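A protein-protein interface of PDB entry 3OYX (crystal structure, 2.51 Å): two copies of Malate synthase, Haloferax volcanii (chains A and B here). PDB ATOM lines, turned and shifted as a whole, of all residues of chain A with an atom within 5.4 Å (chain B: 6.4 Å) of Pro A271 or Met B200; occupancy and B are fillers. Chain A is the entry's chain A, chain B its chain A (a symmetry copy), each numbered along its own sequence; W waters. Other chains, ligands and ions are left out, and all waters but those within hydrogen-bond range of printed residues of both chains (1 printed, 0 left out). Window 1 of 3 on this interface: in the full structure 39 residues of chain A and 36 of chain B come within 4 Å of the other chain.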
ATOM      1  N   ARG A  12     -19.291 -18.787 -20.262  1.00  0.00           N
ATOM      2  CA  ARG A  12     -19.296 -17.351 -19.950  1.00  0.00           C
ATOM      3  C   ARG A  12     -19.894 -17.163 -18.602  1.00  0.00           C
ATOM      4  O   ARG A  12     -19.572 -16.212 -17.899  1.00  0.00           O
ATOM      5  CB  ARG A  12     -20.214 -16.570 -20.895  1.00  0.00           C
ATOM      6  CG  ARG A  12     -19.905 -16.639 -22.377  1.00  0.00           C
ATOM      7  CD  ARG A  12     -21.041 -16.100 -23.153  1.00  0.00           C
ATOM      8  NE  ARG A  12     -22.086 -17.108 -23.081  1.00  0.00           N
ATOM      9  CZ  ARG A  12     -23.263 -17.051 -23.688  1.00  0.00           C
ATOM     10  NH1 ARG A  12     -23.569 -15.987 -24.433  1.00  0.00           N
ATOM     11  NH2 ARG A  12     -24.122 -18.054 -23.534  1.00  0.00           N
ATOM     12  N   MET A 245     -14.715  -8.225 -15.930  1.00  0.00           N
ATOM     13  CA  MET A 245     -14.748  -9.199 -17.030  1.00  0.00           C
ATOM     14  C   MET A 245     -13.835  -8.795 -18.185  1.00  0.00           C
ATOM     15  O   MET A 245     -13.171  -9.620 -18.828  1.00  0.00           O
ATOM     16  CB  MET A 245     -16.159  -9.398 -17.560  1.00  0.00           C
ATOM     17  CG  MET A 245     -17.122  -9.871 -16.506  1.00  0.00           C
ATOM     18  SD  MET A 245     -18.722 -10.286 -17.253  1.00  0.00           S
ATOM     19  CE  MET A 245     -19.623  -8.764 -17.076  1.00  0.00           C
ATOM     20  N   THR A 246     -13.818  -7.497 -18.468  1.00  0.00           N
ATOM     21  CA  THR A 246     -13.033  -6.990 -19.559  1.00  0.00           C
ATOM     22  C   THR A 246     -11.605  -7.296 -19.168  1.00  0.00           C
ATOM     23  O   THR A 246     -10.813  -7.743 -19.993  1.00  0.00           O
ATOM     24  CB  THR A 246     -13.323  -5.496 -19.740  1.00  0.00           C
ATOM     25  OG1 THR A 246     -14.552  -5.399 -20.475  1.00  0.00           O
ATOM     26  CG2 THR A 246     -12.204  -4.800 -20.463  1.00  0.00           C
ATOM     27  N   GLN A 249     -10.823 -11.027 -19.483  1.00  0.00           N
ATOM     28  CA  GLN A 249     -10.844 -11.402 -20.907  1.00  0.00           C
ATOM     29  C   GLN A 249      -9.489 -11.086 -21.473  1.00  0.00           C
ATOM     30  O   GLN A 249      -9.030 -11.758 -22.377  1.00  0.00           O
ATOM     31  CB  GLN A 249     -11.960 -10.682 -21.696  1.00  0.00           C
ATOM     32  CG  GLN A 249     -13.384 -11.232 -21.426  1.00  0.00           C
ATOM     33  CD  GLN A 249     -14.515 -10.218 -21.696  1.00  0.00           C
ATOM     34  OE1 GLN A 249     -14.342  -9.240 -22.464  1.00  0.00           O
ATOM     35  NE2 GLN A 249     -15.693 -10.461 -21.075  1.00  0.00           N
ATOM     36  N   ALA A 250      -8.822 -10.100 -20.906  1.00  0.00           N
ATOM     37  CA  ALA A 250      -7.452  -9.781 -21.315  1.00  0.00           C
ATOM     38  C   ALA A 250      -6.435 -10.852 -20.837  1.00  0.00           C
ATOM     39  O   ALA A 250      -5.277 -10.847 -21.240  1.00  0.00           O
ATOM     40  CB  ALA A 250      -7.048  -8.378 -20.780  1.00  0.00           C
ATOM     41  N   GLY A 252      -7.406 -14.144 -20.784  1.00  0.00           N
ATOM     42  CA  GLY A 252      -7.877 -15.372 -21.415  1.00  0.00           C
ATOM     43  C   GLY A 252      -8.814 -16.083 -20.455  1.00  0.00           C
ATOM     44  O   GLY A 252      -9.120 -17.245 -20.646  1.00  0.00           O
ATOM     45  N   LEU A 254     -12.353 -16.257 -19.772  1.00  0.00           N
ATOM     46  CA  LEU A 254     -13.565 -15.772 -20.459  1.00  0.00           C
ATOM     47  C   LEU A 254     -14.907 -16.002 -19.741  1.00  0.00           C
ATOM     48  O   LEU A 254     -15.960 -15.630 -20.256  1.00  0.00           O
ATOM     49  CB  LEU A 254     -13.643 -16.298 -21.908  1.00  0.00           C
ATOM     50  CG  LEU A 254     -12.406 -16.004 -22.747  1.00  0.00           C
ATOM     51  CD1 LEU A 254     -12.562 -16.649 -24.132  1.00  0.00           C
ATOM     52  CD2 LEU A 254     -12.082 -14.492 -22.906  1.00  0.00           C
ATOM     53  N   GLU A 266     -25.515  -9.797 -17.835  1.00  0.00           N
ATOM     54  CA  GLU A 266     -24.296  -9.030 -18.064  1.00  0.00           C
ATOM     55  C   GLU A 266     -23.094  -9.897 -18.494  1.00  0.00           C
ATOM     56  O   GLU A 266     -22.330  -9.550 -19.398  1.00  0.00           O
ATOM     57  CB  GLU A 266     -23.964  -8.292 -16.779  1.00  0.00           C
ATOM     58  CG  GLU A 266     -24.950  -7.187 -16.489  1.00  0.00           C
ATOM     59  CD  GLU A 266     -24.542  -5.925 -17.227  1.00  0.00           C
ATOM     60  OE1 GLU A 266     -23.440  -5.388 -16.906  1.00  0.00           O
ATOM     61  OE2 GLU A 266     -25.289  -5.515 -18.145  1.00  0.00           O
ATOM     62  N   ALA A 267     -22.944 -11.042 -17.839  1.00  0.00           N
ATOM     63  CA  ALA A 267     -21.830 -11.913 -18.077  1.00  0.00           C
ATOM     64  C   ALA A 267     -22.031 -12.644 -19.400  1.00  0.00           C
ATOM     65  O   ALA A 267     -21.073 -12.942 -20.122  1.00  0.00           O
ATOM     66  CB  ALA A 267     -21.651 -12.874 -16.890  1.00  0.00           C
ATOM     67  N   ASN A 268     -23.279 -12.913 -19.757  1.00  0.00           N
ATOM     68  CA  ASN A 268     -23.578 -13.655 -21.002  1.00  0.00           C
ATOM     69  C   ASN A 268     -23.279 -12.795 -22.223  1.00  0.00           C
ATOM     70  O   ASN A 268     -22.981 -13.293 -23.313  1.00  0.00           O
ATOM     71  CB  ASN A 268     -25.018 -14.150 -20.984  1.00  0.00           C
ATOM     72  CG  ASN A 268     -25.148 -15.639 -20.695  1.00  0.00           C
ATOM     73  OD1 ASN A 268     -24.247 -16.404 -20.945  1.00  0.00           O
ATOM     74  ND2 ASN A 268     -26.319 -16.061 -20.258  1.00  0.00           N
ATOM     75  N   THR A 269     -23.264 -11.487 -21.978  1.00  0.00           N
ATOM     76  CA  THR A 269     -23.244 -10.481 -23.034  1.00  0.00           C
ATOM     77  C   THR A 269     -21.820  -9.943 -23.222  1.00  0.00           C
ATOM     78  O   THR A 269     -21.319  -9.767 -24.344  1.00  0.00           O
ATOM     79  CB  THR A 269     -24.263  -9.324 -22.676  1.00  0.00           C
ATOM     80  OG1 THR A 269     -25.602  -9.855 -22.612  1.00  0.00           O
ATOM     81  CG2 THR A 269     -24.223  -8.208 -23.672  1.00  0.00           C
ATOM     82  N   SER A 270     -21.170  -9.693 -22.091  1.00  0.00           N
ATOM     83  CA  SER A 270     -19.909  -9.001 -22.127  1.00  0.00           C
ATOM     84  C   SER A 270     -18.840  -9.575 -23.084  1.00  0.00           C
ATOM     85  O   SER A 270     -18.226  -8.788 -23.770  1.00  0.00           O
ATOM     86  CB  SER A 270     -19.377  -8.807 -20.719  1.00  0.00           C
ATOM     87  OG  SER A 270     -17.982  -8.684 -20.813  1.00  0.00           O
ATOM     88  N   PRO A 271     -18.612 -10.911 -23.146  1.00  0.00           N
ATOM     89  CA  PRO A 271     -17.544 -11.363 -24.059  1.00  0.00           C
ATOM     90  C   PRO A 271     -17.923 -11.421 -25.550  1.00  0.00           C
ATOM     91  O   PRO A 271     -17.050 -11.625 -26.436  1.00  0.00           O
ATOM     92  CB  PRO A 271     -17.196 -12.768 -23.541  1.00  0.00           C
ATOM     93  CG  PRO A 271     -18.430 -13.227 -22.847  1.00  0.00           C
ATOM     94  CD  PRO A 271     -19.131 -12.018 -22.311  1.00  0.00           C
ATOM     95  N   LEU A 272     -19.226 -11.282 -25.817  1.00  0.00           N
ATOM     96  CA  LEU A 272     -19.733 -11.183 -27.193  1.00  0.00           C
ATOM     97  C   LEU A 272     -19.308  -9.834 -27.793  1.00  0.00           C
ATOM     98  O   LEU A 272     -19.262  -8.830 -27.078  1.00  0.00           O
ATOM     99  CB  LEU A 272     -21.249 -11.337 -27.205  1.00  0.00           C
ATOM    100  CG  LEU A 272     -21.792 -12.680 -26.711  1.00  0.00           C
ATOM    101  CD1 LEU A 272     -23.288 -12.709 -27.037  1.00  0.00           C
ATOM    102  CD2 LEU A 272     -21.080 -13.903 -27.328  1.00  0.00           C
ATOM    103  N   PRO A 273     -18.951  -9.795 -29.085  1.00  0.00           N
ATOM    104  CA  PRO A 273     -18.500  -8.489 -29.643  1.00  0.00           C
ATOM    105  C   PRO A 273     -19.594  -7.406 -29.663  1.00  0.00           C
ATOM    106  O   PRO A 273     -20.764  -7.752 -29.698  1.00  0.00           O
ATOM    107  CB  PRO A 273     -18.031  -8.857 -31.041  1.00  0.00           C
ATOM    108  CG  PRO A 273     -17.653 -10.440 -30.917  1.00  0.00           C
ATOM    109  CD  PRO A 273     -18.756 -10.932 -30.017  1.00  0.00           C
ATOM    110  N   THR B 194      -1.305 -14.815 -26.852  1.00  0.00           N
ATOM    111  CA  THR B 194      -2.645 -14.256 -26.666  1.00  0.00           C
ATOM    112  C   THR B 194      -3.652 -15.218 -27.172  1.00  0.00           C
ATOM    113  O   THR B 194      -4.617 -15.504 -26.481  1.00  0.00           O
ATOM    114  CB  THR B 194      -2.833 -12.893 -27.370  1.00  0.00           C
ATOM    115  OG1 THR B 194      -1.985 -11.968 -26.717  1.00  0.00           O
ATOM    116  CG2 THR B 194      -4.298 -12.334 -27.222  1.00  0.00           C
ATOM    117  N   ARG B 198      -6.338 -17.723 -25.258  1.00  0.00           N
ATOM    118  CA  ARG B 198      -7.693 -17.258 -25.673  1.00  0.00           C
ATOM    119  C   ARG B 198      -8.066 -15.932 -25.035  1.00  0.00           C
ATOM    120  O   ARG B 198      -9.172 -15.742 -24.562  1.00  0.00           O
ATOM    121  CB  ARG B 198      -8.779 -18.316 -25.443  1.00  0.00           C
ATOM    122  CG  ARG B 198      -8.315 -19.759 -25.796  1.00  0.00           C
ATOM    123  CD  ARG B 198      -9.370 -20.841 -25.861  1.00  0.00           C
ATOM    124  NE  ARG B 198     -10.142 -20.898 -24.623  1.00  0.00           N
ATOM    125  CZ  ARG B 198     -11.309 -21.530 -24.505  1.00  0.00           C
ATOM    126  NH1 ARG B 198     -11.809 -22.192 -25.557  1.00  0.00           N
ATOM    127  NH2 ARG B 198     -11.969 -21.500 -23.341  1.00  0.00           N
ATOM    128  N   ALA B 199      -7.128 -15.012 -24.985  1.00  0.00           N
ATOM    129  CA  ALA B 199      -7.410 -13.700 -24.426  1.00  0.00           C
ATOM    130  C   ALA B 199      -8.052 -12.836 -25.537  1.00  0.00           C
ATOM    131  O   ALA B 199      -7.876 -13.116 -26.721  1.00  0.00           O
ATOM    132  CB  ALA B 199      -6.101 -13.068 -23.918  1.00  0.00           C
ATOM    133  N   MET B 200      -8.821 -11.821 -25.165  1.00  0.00           N
ATOM    134  CA  MET B 200      -9.334 -10.857 -26.114  1.00  0.00           C
ATOM    135  C   MET B 200      -9.301  -9.491 -25.460  1.00  0.00           C
ATOM    136  O   MET B 200      -9.300  -9.379 -24.249  1.00  0.00           O
ATOM    137  CB  MET B 200     -10.693 -11.257 -26.677  1.00  0.00           C
ATOM    138  CG  MET B 200     -11.863 -11.311 -25.721  1.00  0.00           C
ATOM    139  SD  MET B 200     -13.193 -12.221 -26.550  1.00  0.00           S
ATOM    140  CE  MET B 200     -14.189 -12.487 -25.132  1.00  0.00           C
ATOM    141  N   THR B 201      -9.131  -8.449 -26.251  1.00  0.00           N
ATOM    142  CA  THR B 201      -9.242  -7.084 -25.743  1.00  0.00           C
ATOM    143  C   THR B 201     -10.172  -6.355 -26.698  1.00  0.00           C
ATOM    144  O   THR B 201     -10.262  -6.755 -27.879  1.00  0.00           O
ATOM    145  CB  THR B 201      -7.899  -6.346 -25.830  1.00  0.00           C
ATOM    146  OG1 THR B 201      -7.423  -6.509 -27.159  1.00  0.00           O
ATOM    147  CG2 THR B 201      -6.893  -6.883 -24.854  1.00  0.00           C
ATOM    148  N   PRO B 202     -10.816  -5.267 -26.215  1.00  0.00           N
ATOM    149  CA  PRO B 202     -11.763  -4.515 -27.051  1.00  0.00           C
ATOM    150  C   PRO B 202     -11.102  -3.930 -28.290  1.00  0.00           C
ATOM    151  O   PRO B 202     -11.639  -4.158 -29.376  1.00  0.00           O
ATOM    152  CB  PRO B 202     -12.279  -3.427 -26.114  1.00  0.00           C
ATOM    153  CG  PRO B 202     -12.119  -4.057 -24.719  1.00  0.00           C
ATOM    154  CD  PRO B 202     -10.744  -4.670 -24.864  1.00  0.00           C
ATOM    155  N   GLY B 204      -8.530  -5.143 -29.742  1.00  0.00           N
ATOM    156  CA  GLY B 204      -7.738  -6.201 -30.398  1.00  0.00           C
ATOM    157  C   GLY B 204      -6.248  -5.864 -30.311  1.00  0.00           C
ATOM    158  O   GLY B 204      -5.461  -6.486 -31.017  1.00  0.00           O
ATOM    159  N   GLU B 205      -5.844  -4.869 -29.496  1.00  0.00           N
ATOM    160  CA  GLU B 205      -4.401  -4.607 -29.199  1.00  0.00           C
ATOM    161  C   GLU B 205      -3.949  -5.691 -28.187  1.00  0.00           C
ATOM    162  O   GLU B 205      -4.766  -6.259 -27.475  1.00  0.00           O
ATOM    163  CB  GLU B 205      -4.106  -3.170 -28.692  1.00  0.00           C
ATOM    164  CG  GLU B 205      -4.023  -2.970 -27.143  1.00  0.00           C
ATOM    165  CD  GLU B 205      -3.098  -1.799 -26.602  1.00  0.00           C
ATOM    166  OE1 GLU B 205      -1.827  -1.903 -26.577  1.00  0.00           O
ATOM    167  OE2 GLU B 205      -3.658  -0.781 -26.119  1.00  0.00           O
ATOM    168  N   PRO B 207      -2.890  -7.804 -24.996  1.00  0.00           N
ATOM    169  CA  PRO B 207      -2.652  -7.529 -23.573  1.00  0.00           C
ATOM    170  C   PRO B 207      -1.144  -7.361 -23.268  1.00  0.00           C
ATOM    171  O   PRO B 207      -0.254  -7.821 -24.034  1.00  0.00           O
ATOM    172  CB  PRO B 207      -3.168  -8.794 -22.862  1.00  0.00           C
ATOM    173  CG  PRO B 207      -3.928  -9.562 -23.891  1.00  0.00           C
ATOM    174  CD  PRO B 207      -3.343  -9.183 -25.223  1.00  0.00           C
ATOM    175  N   ALA B 394      -4.978 -15.151 -33.487  1.00  0.00           N
ATOM    176  CA  ALA B 394      -5.164 -14.283 -32.280  1.00  0.00           C
ATOM    177  C   ALA B 394      -6.354 -13.272 -32.265  1.00  0.00           C
ATOM    178  O   ALA B 394      -6.633 -12.688 -31.209  1.00  0.00           O
ATOM    179  CB  ALA B 394      -3.839 -13.578 -31.828  1.00  0.00           C
ATOM    180  N   THR B 397     -10.905 -15.310 -31.587  1.00  0.00           N
ATOM    181  CA  THR B 397     -11.459 -15.773 -30.347  1.00  0.00           C
ATOM    182  C   THR B 397     -12.899 -15.266 -30.108  1.00  0.00           C
ATOM    183  O   THR B 397     -13.749 -16.081 -29.763  1.00  0.00           O
ATOM    184  CB  THR B 397     -10.463 -15.449 -29.219  1.00  0.00           C
ATOM    185  OG1 THR B 397      -9.266 -16.160 -29.512  1.00  0.00           O
ATOM    186  CG2 THR B 397     -10.983 -15.842 -27.870  1.00  0.00           C
ATOM    187  N   PRO B 398     -13.181 -13.949 -30.307  1.00  0.00           N
ATOM    188  CA  PRO B 398     -14.529 -13.521 -29.978  1.00  0.00           C
ATOM    189  C   PRO B 398     -15.492 -14.231 -30.891  1.00  0.00           C
ATOM    190  O   PRO B 398     -16.600 -14.550 -30.476  1.00  0.00           O
ATOM    191  CB  PRO B 398     -14.516 -12.027 -30.225  1.00  0.00           C
ATOM    192  CG  PRO B 398     -13.091 -11.630 -30.243  1.00  0.00           C
ATOM    193  CD  PRO B 398     -12.359 -12.821 -30.780  1.00  0.00           C
ATOM    194  N   ILE B 399     -15.034 -14.581 -32.088  1.00  0.00           N
ATOM    195  CA  ILE B 399     -15.855 -15.351 -33.041  1.00  0.00           C
ATOM    196  C   ILE B 399     -15.979 -16.850 -32.750  1.00  0.00           C
ATOM    197  O   ILE B 399     -17.071 -17.392 -32.890  1.00  0.00           O
ATOM    198  CB  ILE B 399     -15.380 -15.164 -34.517  1.00  0.00           C
ATOM    199  CG1 ILE B 399     -15.276 -13.667 -34.872  1.00  0.00           C
ATOM    200  CG2 ILE B 399     -16.275 -15.957 -35.471  1.00  0.00           C
ATOM    201  CD1 ILE B 399     -16.550 -12.811 -34.536  1.00  0.00           C
ATOM    202  N   LEU B 401     -15.778 -18.016 -29.785  1.00  0.00           N
ATOM    203  CA  LEU B 401     -16.735 -17.898 -28.689  1.00  0.00           C
ATOM    204  C   LEU B 401     -18.170 -17.698 -29.227  1.00  0.00           C
ATOM    205  O   LEU B 401     -19.096 -18.420 -28.863  1.00  0.00           O
ATOM    206  CB  LEU B 401     -16.366 -16.812 -27.667  1.00  0.00           C
ATOM    207  CG  LEU B 401     -17.525 -16.581 -26.681  1.00  0.00           C
ATOM    208  CD1 LEU B 401     -17.309 -17.273 -25.384  1.00  0.00           C
ATOM    209  CD2 LEU B 401     -17.743 -15.143 -26.374  1.00  0.00           C
HETATM  210  O   HOH W   1     -10.076  -7.381 -22.580  1.00  0.00           O
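The backbone carbonyl oxygen (O) of Gln A249 sits at hydrogen-bond distance from the backbone NH (N) of Met B200 (2.8 Å). The backbone carbonyl oxygen (O) of Met B200 sits at hydrogen-bond distance from the backbone NH (N) of Ala A250 (3.5 Å).
The backbone carbonyl oxygen (O) of Met A245 sits close to the side-chain amide nitrogen (NE2) of Gln A249. The side-chain amide nitrogen (NE2) of Gln A249 is in hydrogen-bond range of the side-chain hydroxyl (OG) of Ser A270 (2.9 Å). The backbone NH (N) of Ala B199 is in hydrogen-bond range of the backbone carbonyl oxygen (O) of Thr B194 (3.0 Å).
Among the printed residues, merely in contact across the chains: Gln A249 with Ala B199 (3.3 Å), Ala A250 with Ala B199 (3.6 Å), Ala A250 with Pro B207 (3.2 Å), Gly A252 with Arg B198 (3.4 Å), Gly A252 with Ala B199 (3.5 Å), Leu A254 with Arg B198 (3.5 Å), Leu A254 with Met B200 (3.7 Å), Pro A271 with Met B200 (3.3 Å), Pro A271 with Leu B401 (3.6 Å), Leu A272 with Leu B401 (3.7 Å) and Pro A273 with Pro B398 (3.6 Å).
Thr A246 touches none of the printed residues of chain B. Pro A271 touches just these residues of chain B: Met B200 (3.3 Å) and Leu B401 (3.6 Å). Of the printed residues of chain B, Leu A272 touches Leu B401 (3.7 Å). Printed residues of chain A within 4 Å of Arg B198: Gly A252 (3.4 Å) and Leu A254 (3.5 Å). Met B200 touches just these residues of chain A: Gln A249 (2.8 Å), Ala A250 (3.5 Å), Leu A254 (3.7 Å) and Pro A271 (3.3 Å). Of the printed residues of chain A, Pro B207 touches Ala A250 (3.2 Å). Ala B394 touches none of the printed residues of chain A. Printed residues of chain A within 4 Å of Leu B401: Pro A271 (3.6 Å) and Leu A272 (3.7 Å). The nearest residue of chain A that does not touch Met B200 is Thr A246 (4.8 Å). The nearest printed residue of chain A that does not touch Arg B198 is Gln A249 (4.5 Å).
Hydrophobic or aromatic side chains of chain A that line the printed part of chain B: Leu A254, Pro A271, Leu A272 and Pro A273. Printed residues of chain B that touch a printed residue of chain A: Arg B198, Ala B199, Met B200, Pro B207, Pro B398 and Leu B401. Along chain B the printed residues that touch a printed residue of chain A span positions 198 to 401.
No position is printed for both chains.
Water W1 lies within hydrogen-bond range of the backbone carbonyl oxygen of Thr A246, the backbone carbonyl oxygen of Met B200 and the backbone NH of Ala A250.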
